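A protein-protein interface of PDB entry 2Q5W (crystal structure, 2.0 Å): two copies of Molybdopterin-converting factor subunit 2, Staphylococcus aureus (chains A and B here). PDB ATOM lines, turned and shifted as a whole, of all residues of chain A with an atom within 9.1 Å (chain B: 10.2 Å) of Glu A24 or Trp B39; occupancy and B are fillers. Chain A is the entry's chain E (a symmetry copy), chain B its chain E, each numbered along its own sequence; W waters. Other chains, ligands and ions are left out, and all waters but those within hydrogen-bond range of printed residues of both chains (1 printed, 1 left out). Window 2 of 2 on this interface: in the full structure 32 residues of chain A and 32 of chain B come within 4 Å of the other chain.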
ATOM      1  N   GLU A  19     -30.807 -10.661  -7.733  1.00  0.00           N
ATOM      2  CA  GLU A  19     -30.948  -9.231  -7.620  1.00  0.00           C
ATOM      3  C   GLU A  19     -29.817  -8.615  -6.770  1.00  0.00           C
ATOM      4  O   GLU A  19     -29.319  -7.556  -7.091  1.00  0.00           O
ATOM      5  CB  GLU A  19     -32.299  -8.848  -7.003  1.00  0.00           C
ATOM      6  CG  GLU A  19     -33.504  -9.365  -7.791  1.00  0.00           C
ATOM      7  CD  GLU A  19     -34.863  -9.002  -7.170  1.00  0.00           C
ATOM      8  OE1 GLU A  19     -34.993  -9.075  -5.903  1.00  0.00           O
ATOM      9  OE2 GLU A  19     -35.802  -8.685  -7.958  1.00  0.00           O
ATOM     10  N   THR A  21     -26.749  -9.591  -6.588  1.00  0.00           N
ATOM     11  CA  THR A  21     -25.519  -9.630  -7.366  1.00  0.00           C
ATOM     12  C   THR A  21     -25.505  -8.722  -8.607  1.00  0.00           C
ATOM     13  O   THR A  21     -24.448  -8.455  -9.149  1.00  0.00           O
ATOM     14  CB  THR A  21     -25.151 -11.049  -7.813  1.00  0.00           C
ATOM     15  OG1 THR A  21     -26.055 -11.473  -8.835  1.00  0.00           O
ATOM     16  CG2 THR A  21     -25.147 -12.019  -6.605  1.00  0.00           C
ATOM     17  N   ILE A  22     -26.655  -8.229  -9.044  1.00  0.00           N
ATOM     18  CA  ILE A  22     -26.732  -7.456 -10.253  1.00  0.00           C
ATOM     19  C   ILE A  22     -26.383  -6.005 -10.046  1.00  0.00           C
ATOM     20  O   ILE A  22     -26.821  -5.410  -9.105  1.00  0.00           O
ATOM     21  CB  ILE A  22     -28.163  -7.481 -10.845  1.00  0.00           C
ATOM     22  CG1 ILE A  22     -28.544  -8.881 -11.218  1.00  0.00           C
ATOM     23  CG2 ILE A  22     -28.281  -6.520 -12.029  1.00  0.00           C
ATOM     24  CD1 ILE A  22     -30.030  -8.922 -11.738  1.00  0.00           C
ATOM     25  N   ASN A  23     -25.643  -5.433 -10.997  1.00  0.00           N
ATOM     26  CA  ASN A  23     -25.485  -3.989 -11.124  1.00  0.00           C
ATOM     27  C   ASN A  23     -25.138  -3.725 -12.572  1.00  0.00           C
ATOM     28  O   ASN A  23     -24.947  -4.673 -13.327  1.00  0.00           O
ATOM     29  CB  ASN A  23     -24.456  -3.415 -10.130  1.00  0.00           C
ATOM     30  CG  ASN A  23     -23.026  -3.912 -10.392  1.00  0.00           C
ATOM     31  OD1 ASN A  23     -22.502  -3.806 -11.505  1.00  0.00           O
ATOM     32  ND2 ASN A  23     -22.416  -4.470  -9.376  1.00  0.00           N
ATOM     33  N   GLU A  24     -25.083  -2.455 -12.960  1.00  0.00           N
ATOM     34  CA  GLU A  24     -24.910  -2.062 -14.360  1.00  0.00           C
ATOM     35  C   GLU A  24     -23.631  -2.518 -15.066  1.00  0.00           C
ATOM     36  O   GLU A  24     -23.547  -2.411 -16.289  1.00  0.00           O
ATOM     37  CB  GLU A  24     -25.053  -0.566 -14.510  1.00  0.00           C
ATOM     38  CG  GLU A  24     -23.946   0.219 -13.823  1.00  0.00           C
ATOM     39  CD  GLU A  24     -24.215   1.713 -13.730  1.00  0.00           C
ATOM     40  OE1 GLU A  24     -24.874   2.329 -14.644  1.00  0.00           O
ATOM     41  OE2 GLU A  24     -23.733   2.282 -12.725  1.00  0.00           O
ATOM     42  N   TYR A  25     -22.645  -3.025 -14.328  1.00  0.00           N
ATOM     43  CA  TYR A  25     -21.423  -3.522 -14.952  1.00  0.00           C
ATOM     44  C   TYR A  25     -21.504  -5.001 -15.219  1.00  0.00           C
ATOM     45  O   TYR A  25     -20.651  -5.540 -15.909  1.00  0.00           O
ATOM     46  CB  TYR A  25     -20.207  -3.292 -14.037  1.00  0.00           C
ATOM     47  CG  TYR A  25     -19.702  -1.891 -13.999  1.00  0.00           C
ATOM     48  CD1 TYR A  25     -20.175  -0.993 -13.077  1.00  0.00           C
ATOM     49  CD2 TYR A  25     -18.789  -1.453 -14.915  1.00  0.00           C
ATOM     50  CE1 TYR A  25     -19.702   0.287 -13.025  1.00  0.00           C
ATOM     51  CE2 TYR A  25     -18.324  -0.152 -14.895  1.00  0.00           C
ATOM     52  CZ  TYR A  25     -18.768   0.702 -13.937  1.00  0.00           C
ATOM     53  OH  TYR A  25     -18.277   1.971 -13.884  1.00  0.00           O
ATOM     54  N   GLN A  26     -22.508  -5.677 -14.656  1.00  0.00           N
ATOM     55  CA  GLN A  26     -22.592  -7.140 -14.760  1.00  0.00           C
ATOM     56  C   GLN A  26     -23.462  -7.552 -15.925  1.00  0.00           C
ATOM     57  O   GLN A  26     -24.631  -7.127 -16.071  1.00  0.00           O
ATOM     58  CB  GLN A  26     -23.123  -7.746 -13.456  1.00  0.00           C
ATOM     59  CG  GLN A  26     -22.459  -7.266 -12.194  1.00  0.00           C
ATOM     60  CD  GLN A  26     -20.942  -7.539 -12.104  1.00  0.00           C
ATOM     61  OE1 GLN A  26     -20.154  -6.958 -12.846  1.00  0.00           O
ATOM     62  NE2 GLN A  26     -20.541  -8.378 -11.145  1.00  0.00           N
ATOM     63  N   GLY A  27     -22.880  -8.369 -16.798  1.00  0.00           N
ATOM     64  CA  GLY A  27     -23.594  -8.826 -17.961  1.00  0.00           C
ATOM     65  C   GLY A  27     -23.978 -10.278 -17.864  1.00  0.00           C
ATOM     66  O   GLY A  27     -24.707 -10.789 -18.686  1.00  0.00           O
ATOM     67  N   ALA A  28     -23.510 -10.946 -16.838  1.00  0.00           N
ATOM     68  CA  ALA A  28     -23.817 -12.344 -16.682  1.00  0.00           C
ATOM     69  C   ALA A  28     -24.125 -12.652 -15.224  1.00  0.00           C
ATOM     70  O   ALA A  28     -23.451 -12.168 -14.325  1.00  0.00           O
ATOM     71  CB  ALA A  28     -22.640 -13.176 -17.178  1.00  0.00           C
ATOM     72  N   ILE A  76     -19.511 -10.822  -8.093  1.00  0.00           N
ATOM     73  CA  ILE A  76     -20.204 -10.625  -6.846  1.00  0.00           C
ATOM     74  C   ILE A  76     -20.922 -11.953  -6.550  1.00  0.00           C
ATOM     75  O   ILE A  76     -21.532 -12.529  -7.461  1.00  0.00           O
ATOM     76  CB  ILE A  76     -21.191  -9.489  -6.943  1.00  0.00           C
ATOM     77  CG1 ILE A  76     -20.449  -8.167  -7.242  1.00  0.00           C
ATOM     78  CG2 ILE A  76     -22.005  -9.365  -5.626  1.00  0.00           C
ATOM     79  CD1 ILE A  76     -21.348  -7.067  -7.593  1.00  0.00           C
ATOM     80  N   SER A  98     -22.472 -12.993 -10.185  1.00  0.00           N
ATOM     81  CA  SER A  98     -22.496 -12.033 -11.282  1.00  0.00           C
ATOM     82  C   SER A  98     -21.101 -11.679 -11.730  1.00  0.00           C
ATOM     83  O   SER A  98     -20.131 -11.819 -10.963  1.00  0.00           O
ATOM     84  CB  SER A  98     -23.250 -10.760 -10.870  1.00  0.00           C
ATOM     85  OG  SER A  98     -22.551  -9.993  -9.892  1.00  0.00           O
ATOM     86  N   SER A  99     -20.986 -11.248 -12.988  1.00  0.00           N
ATOM     87  CA  SER A  99     -19.682 -10.888 -13.573  1.00  0.00           C
ATOM     88  C   SER A  99     -19.908 -10.022 -14.824  1.00  0.00           C
ATOM     89  O   SER A  99     -20.974 -10.103 -15.447  1.00  0.00           O
ATOM     90  CB  SER A  99     -18.896 -12.172 -13.954  1.00  0.00           C
ATOM     91  OG  SER A  99     -17.542 -11.846 -14.322  1.00  0.00           O
ATOM     92  N   PRO A 100     -18.936  -9.159 -15.178  1.00  0.00           N
ATOM     93  CA  PRO A 100     -19.116  -8.492 -16.442  1.00  0.00           C
ATOM     94  C   PRO A 100     -19.270  -9.468 -17.595  1.00  0.00           C
ATOM     95  O   PRO A 100     -20.096  -9.239 -18.479  1.00  0.00           O
ATOM     96  CB  PRO A 100     -17.832  -7.683 -16.594  1.00  0.00           C
ATOM     97  CG  PRO A 100     -17.420  -7.374 -15.158  1.00  0.00           C
ATOM     98  CD  PRO A 100     -17.732  -8.675 -14.470  1.00  0.00           C
ATOM     99  N   HIS B  35     -27.564  -9.989 -19.009  1.00  0.00           N
ATOM    100  CA  HIS B  35     -28.112  -8.705 -18.674  1.00  0.00           C
ATOM    101  C   HIS B  35     -27.480  -7.568 -19.483  1.00  0.00           C
ATOM    102  O   HIS B  35     -26.284  -7.583 -19.779  1.00  0.00           O
ATOM    103  CB  HIS B  35     -27.863  -8.398 -17.213  1.00  0.00           C
ATOM    104  CG  HIS B  35     -28.491  -9.383 -16.279  1.00  0.00           C
ATOM    105  ND1 HIS B  35     -29.562  -9.063 -15.477  1.00  0.00           N
ATOM    106  CD2 HIS B  35     -28.190 -10.673 -16.016  1.00  0.00           C
ATOM    107  CE1 HIS B  35     -29.892 -10.129 -14.754  1.00  0.00           C
ATOM    108  NE2 HIS B  35     -29.083 -11.119 -15.071  1.00  0.00           N
ATOM    109  N   VAL B  36     -28.278  -6.537 -19.735  1.00  0.00           N
ATOM    110  CA  VAL B  36     -27.817  -5.351 -20.431  1.00  0.00           C
ATOM    111  C   VAL B  36     -26.826  -4.600 -19.553  1.00  0.00           C
ATOM    112  O   VAL B  36     -27.148  -4.225 -18.411  1.00  0.00           O
ATOM    113  CB  VAL B  36     -29.004  -4.444 -20.825  1.00  0.00           C
ATOM    114  CG1 VAL B  36     -28.525  -3.185 -21.561  1.00  0.00           C
ATOM    115  CG2 VAL B  36     -29.954  -5.202 -21.726  1.00  0.00           C
ATOM    116  N   ARG B  37     -25.615  -4.360 -20.085  1.00  0.00           N
ATOM    117  CA  ARG B  37     -24.594  -3.619 -19.359  1.00  0.00           C
ATOM    118  C   ARG B  37     -24.515  -2.181 -19.798  1.00  0.00           C
ATOM    119  O   ARG B  37     -24.742  -1.826 -20.953  1.00  0.00           O
ATOM    120  CB  ARG B  37     -23.193  -4.196 -19.579  1.00  0.00           C
ATOM    121  CG  ARG B  37     -22.931  -5.491 -18.899  1.00  0.00           C
ATOM    122  CD  ARG B  37     -21.497  -5.870 -19.037  1.00  0.00           C
ATOM    123  NE  ARG B  37     -21.125  -6.198 -20.415  1.00  0.00           N
ATOM    124  CZ  ARG B  37     -19.876  -6.084 -20.899  1.00  0.00           C
ATOM    125  NH1 ARG B  37     -18.871  -5.661 -20.136  1.00  0.00           N
ATOM    126  NH2 ARG B  37     -19.634  -6.383 -22.171  1.00  0.00           N
ATOM    127  N   GLU B  38     -24.130  -1.364 -18.842  1.00  0.00           N
ATOM    128  CA  GLU B  38     -23.782   0.007 -19.061  1.00  0.00           C
ATOM    129  C   GLU B  38     -22.262   0.110 -19.136  1.00  0.00           C
ATOM    130  O   GLU B  38     -21.481  -0.745 -18.605  1.00  0.00           O
ATOM    131  CB  GLU B  38     -24.310   0.848 -17.890  1.00  0.00           C
ATOM    132  CG  GLU B  38     -24.182   2.293 -18.060  1.00  0.00           C
ATOM    133  CD  GLU B  38     -24.768   2.689 -19.354  1.00  0.00           C
ATOM    134  OE1 GLU B  38     -24.035   2.585 -20.414  1.00  0.00           O
ATOM    135  OE2 GLU B  38     -25.974   3.017 -19.271  1.00  0.00           O
ATOM    136  N   TRP B  39     -21.854   1.159 -19.813  1.00  0.00           N
ATOM    137  CA  TRP B  39     -20.502   1.622 -19.864  1.00  0.00           C
ATOM    138  C   TRP B  39     -19.582   0.763 -20.652  1.00  0.00           C
ATOM    139  O   TRP B  39     -18.363   0.845 -20.445  1.00  0.00           O
ATOM    140  CB  TRP B  39     -19.888   1.945 -18.496  1.00  0.00           C
ATOM    141  CG  TRP B  39     -20.715   2.819 -17.699  1.00  0.00           C
ATOM    142  CD1 TRP B  39     -21.314   2.510 -16.525  1.00  0.00           C
ATOM    143  CD2 TRP B  39     -21.070   4.160 -17.996  1.00  0.00           C
ATOM    144  NE1 TRP B  39     -22.017   3.579 -16.065  1.00  0.00           N
ATOM    145  CE2 TRP B  39     -21.883   4.612 -16.948  1.00  0.00           C
ATOM    146  CE3 TRP B  39     -20.790   5.024 -19.054  1.00  0.00           C
ATOM    147  CZ2 TRP B  39     -22.444   5.872 -16.934  1.00  0.00           C
ATOM    148  CZ3 TRP B  39     -21.314   6.276 -19.031  1.00  0.00           C
ATOM    149  CH2 TRP B  39     -22.138   6.698 -17.967  1.00  0.00           C
ATOM    150  N   THR B  40     -20.114   0.043 -21.621  1.00  0.00           N
ATOM    151  CA  THR B  40     -19.244  -0.663 -22.531  1.00  0.00           C
ATOM    152  C   THR B  40     -18.626   0.246 -23.569  1.00  0.00           C
ATOM    153  O   THR B  40     -17.672  -0.154 -24.215  1.00  0.00           O
ATOM    154  CB  THR B  40     -19.946  -1.796 -23.241  1.00  0.00           C
ATOM    155  OG1 THR B  40     -20.961  -1.288 -24.110  1.00  0.00           O
ATOM    156  CG2 THR B  40     -20.552  -2.743 -22.207  1.00  0.00           C
ATOM    157  N   LYS B  41     -19.172   1.442 -23.769  1.00  0.00           N
ATOM    158  CA  LYS B  41     -18.570   2.389 -24.637  1.00  0.00           C
ATOM    159  C   LYS B  41     -18.328   3.669 -23.807  1.00  0.00           C
ATOM    160  O   LYS B  41     -18.704   3.745 -22.644  1.00  0.00           O
ATOM    161  CB  LYS B  41     -19.502   2.669 -25.843  1.00  0.00           C
ATOM    162  CG  LYS B  41     -20.289   1.452 -26.390  1.00  0.00           C
ATOM    163  CD  LYS B  41     -19.534   0.726 -27.504  1.00  0.00           C
ATOM    164  CE  LYS B  41     -20.421  -0.380 -28.169  1.00  0.00           C
ATOM    165  NZ  LYS B  41     -21.092  -1.312 -27.210  1.00  0.00           N
ATOM    166  N   GLY B  42     -17.675   4.647 -24.420  1.00  0.00           N
ATOM    167  CA  GLY B  42     -17.472   5.969 -23.809  1.00  0.00           C
ATOM    168  C   GLY B  42     -18.784   6.748 -23.655  1.00  0.00           C
ATOM    169  O   GLY B  42     -19.020   7.437 -22.653  1.00  0.00           O
ATOM    170  N   VAL B  43     -19.652   6.623 -24.630  1.00  0.00           N
ATOM    171  CA  VAL B  43     -20.936   7.265 -24.580  1.00  0.00           C
ATOM    172  C   VAL B  43     -21.871   6.309 -23.863  1.00  0.00           C
ATOM    173  O   VAL B  43     -21.960   5.136 -24.200  1.00  0.00           O
ATOM    174  CB  VAL B  43     -21.487   7.586 -26.008  1.00  0.00           C
ATOM    175  CG1 VAL B  43     -22.888   8.214 -25.946  1.00  0.00           C
ATOM    176  CG2 VAL B  43     -20.549   8.495 -26.766  1.00  0.00           C
ATOM    177  N   LYS B  44     -22.605   6.823 -22.888  1.00  0.00           N
ATOM    178  CA  LYS B  44     -23.549   6.008 -22.118  1.00  0.00           C
ATOM    179  C   LYS B  44     -24.590   5.294 -23.005  1.00  0.00           C
ATOM    180  O   LYS B  44     -25.128   5.877 -23.940  1.00  0.00           O
ATOM    181  CB  LYS B  44     -24.218   6.880 -21.056  1.00  0.00           C
ATOM    182  CG  LYS B  44     -25.154   6.140 -20.121  1.00  0.00           C
ATOM    183  CD  LYS B  44     -25.928   7.119 -19.221  1.00  0.00           C
ATOM    184  CE  LYS B  44     -26.616   6.388 -18.072  1.00  0.00           C
ATOM    185  NZ  LYS B  44     -26.653   7.248 -16.788  1.00  0.00           N
ATOM    186  N   THR B  45     -24.811   4.011 -22.743  1.00  0.00           N
ATOM    187  CA  THR B  45     -25.901   3.250 -23.367  1.00  0.00           C
ATOM    188  C   THR B  45     -27.209   3.629 -22.680  1.00  0.00           C
ATOM    189  O   THR B  45     -27.328   3.535 -21.462  1.00  0.00           O
ATOM    190  CB  THR B  45     -25.627   1.727 -23.282  1.00  0.00           C
ATOM    191  OG1 THR B  45     -24.329   1.467 -23.848  1.00  0.00           O
ATOM    192  CG2 THR B  45     -26.689   0.896 -24.004  1.00  0.00           C
ATOM    193  N   GLU B  46     -28.168   4.120 -23.469  1.00  0.00           N
ATOM    194  CA  GLU B  46     -29.472   4.526 -22.932  1.00  0.00           C
ATOM    195  C   GLU B  46     -30.289   3.299 -22.700  1.00  0.00           C
ATOM    196  O   GLU B  46     -30.794   3.105 -21.612  1.00  0.00           O
ATOM    197  CB  GLU B  46     -30.206   5.499 -23.869  1.00  0.00           C
ATOM    198  CG  GLU B  46     -29.498   6.844 -24.071  1.00  0.00           C
ATOM    199  CD  GLU B  46     -29.235   7.604 -22.779  1.00  0.00           C
ATOM    200  OE1 GLU B  46     -30.080   7.525 -21.858  1.00  0.00           O
ATOM    201  OE2 GLU B  46     -28.181   8.283 -22.674  1.00  0.00           O
ATOM    202  N   TYR B  47     -30.371   2.449 -23.719  1.00  0.00           N
ATOM    203  CA  TYR B  47     -31.072   1.189 -23.650  1.00  0.00           C
ATOM    204  C   TYR B  47     -30.725   0.390 -24.925  1.00  0.00           C
ATOM    205  O   TYR B  47     -30.033   0.917 -25.799  1.00  0.00           O
ATOM    206  CB  TYR B  47     -32.599   1.392 -23.505  1.00  0.00           C
ATOM    207  CG  TYR B  47     -33.255   2.086 -24.673  1.00  0.00           C
ATOM    208  CD1 TYR B  47     -33.884   1.362 -25.680  1.00  0.00           C
ATOM    209  CD2 TYR B  47     -33.240   3.481 -24.777  1.00  0.00           C
ATOM    210  CE1 TYR B  47     -34.510   2.036 -26.782  1.00  0.00           C
ATOM    211  CE2 TYR B  47     -33.827   4.131 -25.845  1.00  0.00           C
ATOM    212  CZ  TYR B  47     -34.450   3.400 -26.855  1.00  0.00           C
ATOM    213  OH  TYR B  47     -35.041   4.084 -27.898  1.00  0.00           O
ATOM    214  N   LEU B  48     -31.196  -0.860 -25.024  1.00  0.00           N
ATOM    215  CA  LEU B  48     -31.040  -1.668 -26.230  1.00  0.00           C
ATOM    216  C   LEU B  48     -32.422  -1.983 -26.809  1.00  0.00           C
ATOM    217  O   LEU B  48     -33.411  -2.012 -26.069  1.00  0.00           O
ATOM    218  CB  LEU B  48     -30.346  -2.998 -25.951  1.00  0.00           C
ATOM    219  CG  LEU B  48     -28.936  -2.990 -25.366  1.00  0.00           C
ATOM    220  CD1 LEU B  48     -28.383  -4.417 -25.315  1.00  0.00           C
ATOM    221  CD2 LEU B  48     -28.043  -2.138 -26.138  1.00  0.00           C
ATOM    222  N   GLN B  87     -33.925  -2.237 -20.802  1.00  0.00           N
ATOM    223  CA  GLN B  87     -33.197  -1.270 -20.014  1.00  0.00           C
ATOM    224  C   GLN B  87     -31.913  -1.863 -19.425  1.00  0.00           C
ATOM    225  O   GLN B  87     -31.739  -3.046 -19.414  1.00  0.00           O
ATOM    226  CB  GLN B  87     -34.085  -0.763 -18.882  1.00  0.00           C
ATOM    227  CG  GLN B  87     -35.472  -0.349 -19.337  1.00  0.00           C
ATOM    228  CD  GLN B  87     -35.430   0.747 -20.343  1.00  0.00           C
ATOM    229  OE1 GLN B  87     -34.720   1.745 -20.152  1.00  0.00           O
ATOM    230  NE2 GLN B  87     -36.176   0.587 -21.426  1.00  0.00           N
ATOM    231  N   ILE B  88     -31.069  -1.000 -18.851  1.00  0.00           N
ATOM    232  CA  ILE B  88     -29.837  -1.443 -18.199  1.00  0.00           C
ATOM    233  C   ILE B  88     -30.223  -2.468 -17.142  1.00  0.00           C
ATOM    234  O   ILE B  88     -31.170  -2.270 -16.400  1.00  0.00           O
ATOM    235  CB  ILE B  88     -29.045  -0.253 -17.567  1.00  0.00           C
ATOM    236  CG1 ILE B  88     -28.711   0.825 -18.633  1.00  0.00           C
ATOM    237  CG2 ILE B  88     -27.781  -0.733 -16.849  1.00  0.00           C
ATOM    238  CD1 ILE B  88     -28.055   0.309 -19.884  1.00  0.00           C
ATOM    239  N   SER B  89     -29.482  -3.568 -17.112  1.00  0.00           N
ATOM    240  CA  SER B  89     -29.660  -4.671 -16.154  1.00  0.00           C
ATOM    241  C   SER B  89     -30.889  -5.532 -16.373  1.00  0.00           C
ATOM    242  O   SER B  89     -31.065  -6.527 -15.660  1.00  0.00           O
ATOM    243  CB  SER B  89     -29.540  -4.178 -14.702  1.00  0.00           C
ATOM    244  OG  SER B  89     -28.223  -3.674 -14.474  1.00  0.00           O
ATOM    245  N   ASP B  90     -31.704  -5.230 -17.385  1.00  0.00           N
ATOM    246  CA  ASP B  90     -32.786  -6.150 -17.759  1.00  0.00           C
ATOM    247  C   ASP B  90     -32.165  -7.471 -18.238  1.00  0.00           C
ATOM    248  O   ASP B  90     -31.077  -7.490 -18.818  1.00  0.00           O
ATOM    249  CB  ASP B  90     -33.684  -5.600 -18.881  1.00  0.00           C
ATOM    250  CG  ASP B  90     -34.723  -4.581 -18.405  1.00  0.00           C
ATOM    251  OD1 ASP B  90     -34.799  -4.266 -17.211  1.00  0.00           O
ATOM    252  OD2 ASP B  90     -35.466  -4.082 -19.270  1.00  0.00           O
ATOM    253  N   GLU B 126     -27.985  -1.005 -30.181  1.00  0.00           N
ATOM    254  CA  GLU B 126     -27.625  -0.095 -29.097  1.00  0.00           C
ATOM    255  C   GLU B 126     -28.087   1.296 -29.404  1.00  0.00           C
ATOM    256  O   GLU B 126     -27.868   1.795 -30.527  1.00  0.00           O
ATOM    257  CB  GLU B 126     -26.105  -0.004 -28.890  1.00  0.00           C
ATOM    258  CG  GLU B 126     -25.522  -1.295 -28.511  1.00  0.00           C
ATOM    259  CD  GLU B 126     -24.127  -1.209 -27.915  1.00  0.00           C
ATOM    260  OE1 GLU B 126     -23.563  -0.108 -27.781  1.00  0.00           O
ATOM    261  OE2 GLU B 126     -23.621  -2.305 -27.593  1.00  0.00           O
ATOM    262  N   ILE B 127     -28.692   1.934 -28.400  1.00  0.00           N
ATOM    263  CA  ILE B 127     -29.146   3.313 -28.517  1.00  0.00           C
ATOM    264  C   ILE B 127     -28.399   4.188 -27.509  1.00  0.00           C
ATOM    265  O   ILE B 127     -28.310   3.863 -26.325  1.00  0.00           O
ATOM    266  CB  ILE B 127     -30.671   3.437 -28.305  1.00  0.00           C
ATOM    267  CG1 ILE B 127     -31.448   2.787 -29.469  1.00  0.00           C
ATOM    268  CG2 ILE B 127     -31.086   4.918 -28.278  1.00  0.00           C
ATOM    269  CD1 ILE B 127     -31.779   1.494 -29.320  1.00  0.00           C
ATOM    270  N   TRP B 128     -27.853   5.293 -27.988  1.00  0.00           N
ATOM    271  CA  TRP B 128     -27.174   6.219 -27.122  1.00  0.00           C
ATOM    272  C   TRP B 128     -27.662   7.600 -27.469  1.00  0.00           C
ATOM    273  O   TRP B 128     -28.438   7.738 -28.399  1.00  0.00           O
ATOM    274  CB  TRP B 128     -25.662   6.093 -27.253  1.00  0.00           C
ATOM    275  CG  TRP B 128     -25.117   6.343 -28.616  1.00  0.00           C
ATOM    276  CD1 TRP B 128     -24.743   7.546 -29.170  1.00  0.00           C
ATOM    277  CD2 TRP B 128     -24.820   5.341 -29.588  1.00  0.00           C
ATOM    278  NE1 TRP B 128     -24.241   7.337 -30.442  1.00  0.00           N
ATOM    279  CE2 TRP B 128     -24.276   5.990 -30.715  1.00  0.00           C
ATOM    280  CE3 TRP B 128     -24.911   3.953 -29.591  1.00  0.00           C
ATOM    281  CZ2 TRP B 128     -23.889   5.286 -31.863  1.00  0.00           C
ATOM    282  CZ3 TRP B 128     -24.526   3.255 -30.724  1.00  0.00           C
ATOM    283  CH2 TRP B 128     -24.033   3.920 -31.841  1.00  0.00           C
ATOM    284  N   GLU B 129     -27.230   8.604 -26.713  1.00  0.00           N
ATOM    285  CA  GLU B 129     -27.727   9.980 -26.842  1.00  0.00           C
ATOM    286  C   GLU B 129     -28.190  10.457 -28.241  1.00  0.00           C
ATOM    287  O   GLU B 129     -29.385  10.696 -28.433  1.00  0.00           O
ATOM    288  CB  GLU B 129     -26.718  10.982 -26.262  1.00  0.00           C
ATOM    289  CG  GLU B 129     -27.037  12.433 -26.558  1.00  0.00           C
ATOM    290  CD  GLU B 129     -28.502  12.837 -26.327  1.00  0.00           C
ATOM    291  OE1 GLU B 129     -29.068  12.419 -25.305  1.00  0.00           O
ATOM    292  OE2 GLU B 129     -29.060  13.613 -27.163  1.00  0.00           O
HETATM  293  O   HOH W   1     -18.723  -4.426 -17.403  1.00  0.00           O
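The side-chain carboxylate of Glu B38 sits at hydrogen-bond distance from the backbone NH of Thr B45, 2.8 Å away. ND1 of His B35 lies within hydrogen-bond range of O of Ser B89, at 3.0 Å. The backbone NH (N) of Gly A27 sits at hydrogen-bond distance from the backbone carbonyl oxygen (O) of Pro A100 (3.4 Å). The side-chain amide oxygen of Asn A23 lies within hydrogen-bond range of the backbone NH of Tyr A25, 2.9 Å away. The backbone NH (N) of Gly A27 lies within hydrogen-bond range of the backbone carbonyl oxygen (O) of Ser A99 (2.9 Å). The backbone NH (N) of Ser A99 sits close to the side-chain amide nitrogen (NE2) of Gln A26.
Water W1 lies within hydrogen-bond range of O of Tyr A25 (2.7 Å) and NH1 of Arg B37 (3.0 Å).
Printed residues of chain B within 4 Å of Ile A22: His B35 (3.3 Å) and Ser B89 (3.8 Å). Asn A23 touches just one residue of chain B: Ser B89. Glu A24 touches five residues of chain B. Tyr A25 touches one residue of chain B. Ala A28 touches none of the printed residues of chain B. Of chain A, only Glu A24 comes within 4 Å of Glu B38. Of chain A, only Glu A24 (3.4 Å) comes within 4 Å of Trp B39. No residue of chain A comes within 4 Å of Thr B40. Gly B42 touches none of the printed residues of chain A. Of the printed residues of chain A, Ser B89 touches Ile A22, Asn A23 and Glu A24. The nearest residue of chain A that does not touch Trp B39 is Tyr A25 (4.1 Å). The nearest printed residue of chain B that does not touch Ile A22 is Asp B90 (6.5 Å).
Hydrophobic or aromatic side chains of chain A within 4 Å of the printed part of chain B: Ile A22. Hydrophobic or aromatic side chains of chain B that line the printed part of chain A: His B35, Trp B39 and Ile B88. Among the printed residues, no Asp or Glu carboxylate lies within 4 Å of a Lys or Arg side-chain nitrogen of the other chain.
The indole nitrogen (NE1) of Trp B39 sits at hydrogen-bond distance from the side-chain carboxylate (OE1) of Glu A24 (3.4 Å). The backbone NH (N) of Glu B38 lies within hydrogen-bond range of the backbone carbonyl oxygen (O) of Glu A24. The backbone NH of His B35 is in hydrogen-bond range of the backbone carbonyl oxygen of Gly A27 (3.0 Å).
No position is printed for both chains. Of the 14 pairs that touch across the chains among the printed residues, none has its exchanged pair printed and touching as well.
Among the printed residues, merely in contact across the chains: Ile A22 with His B35, Ile A22 with Ser B89, Asn A23 with Ser B89, Glu A24 with Arg B37, Glu A24 with Ile B88, Glu A24 with Ser B89, Tyr A25 with Arg B37, Gln A26 with His B35, Gln A26 with Arg B37, Gly A27 with Arg B37 and Pro A100 with Arg B37.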
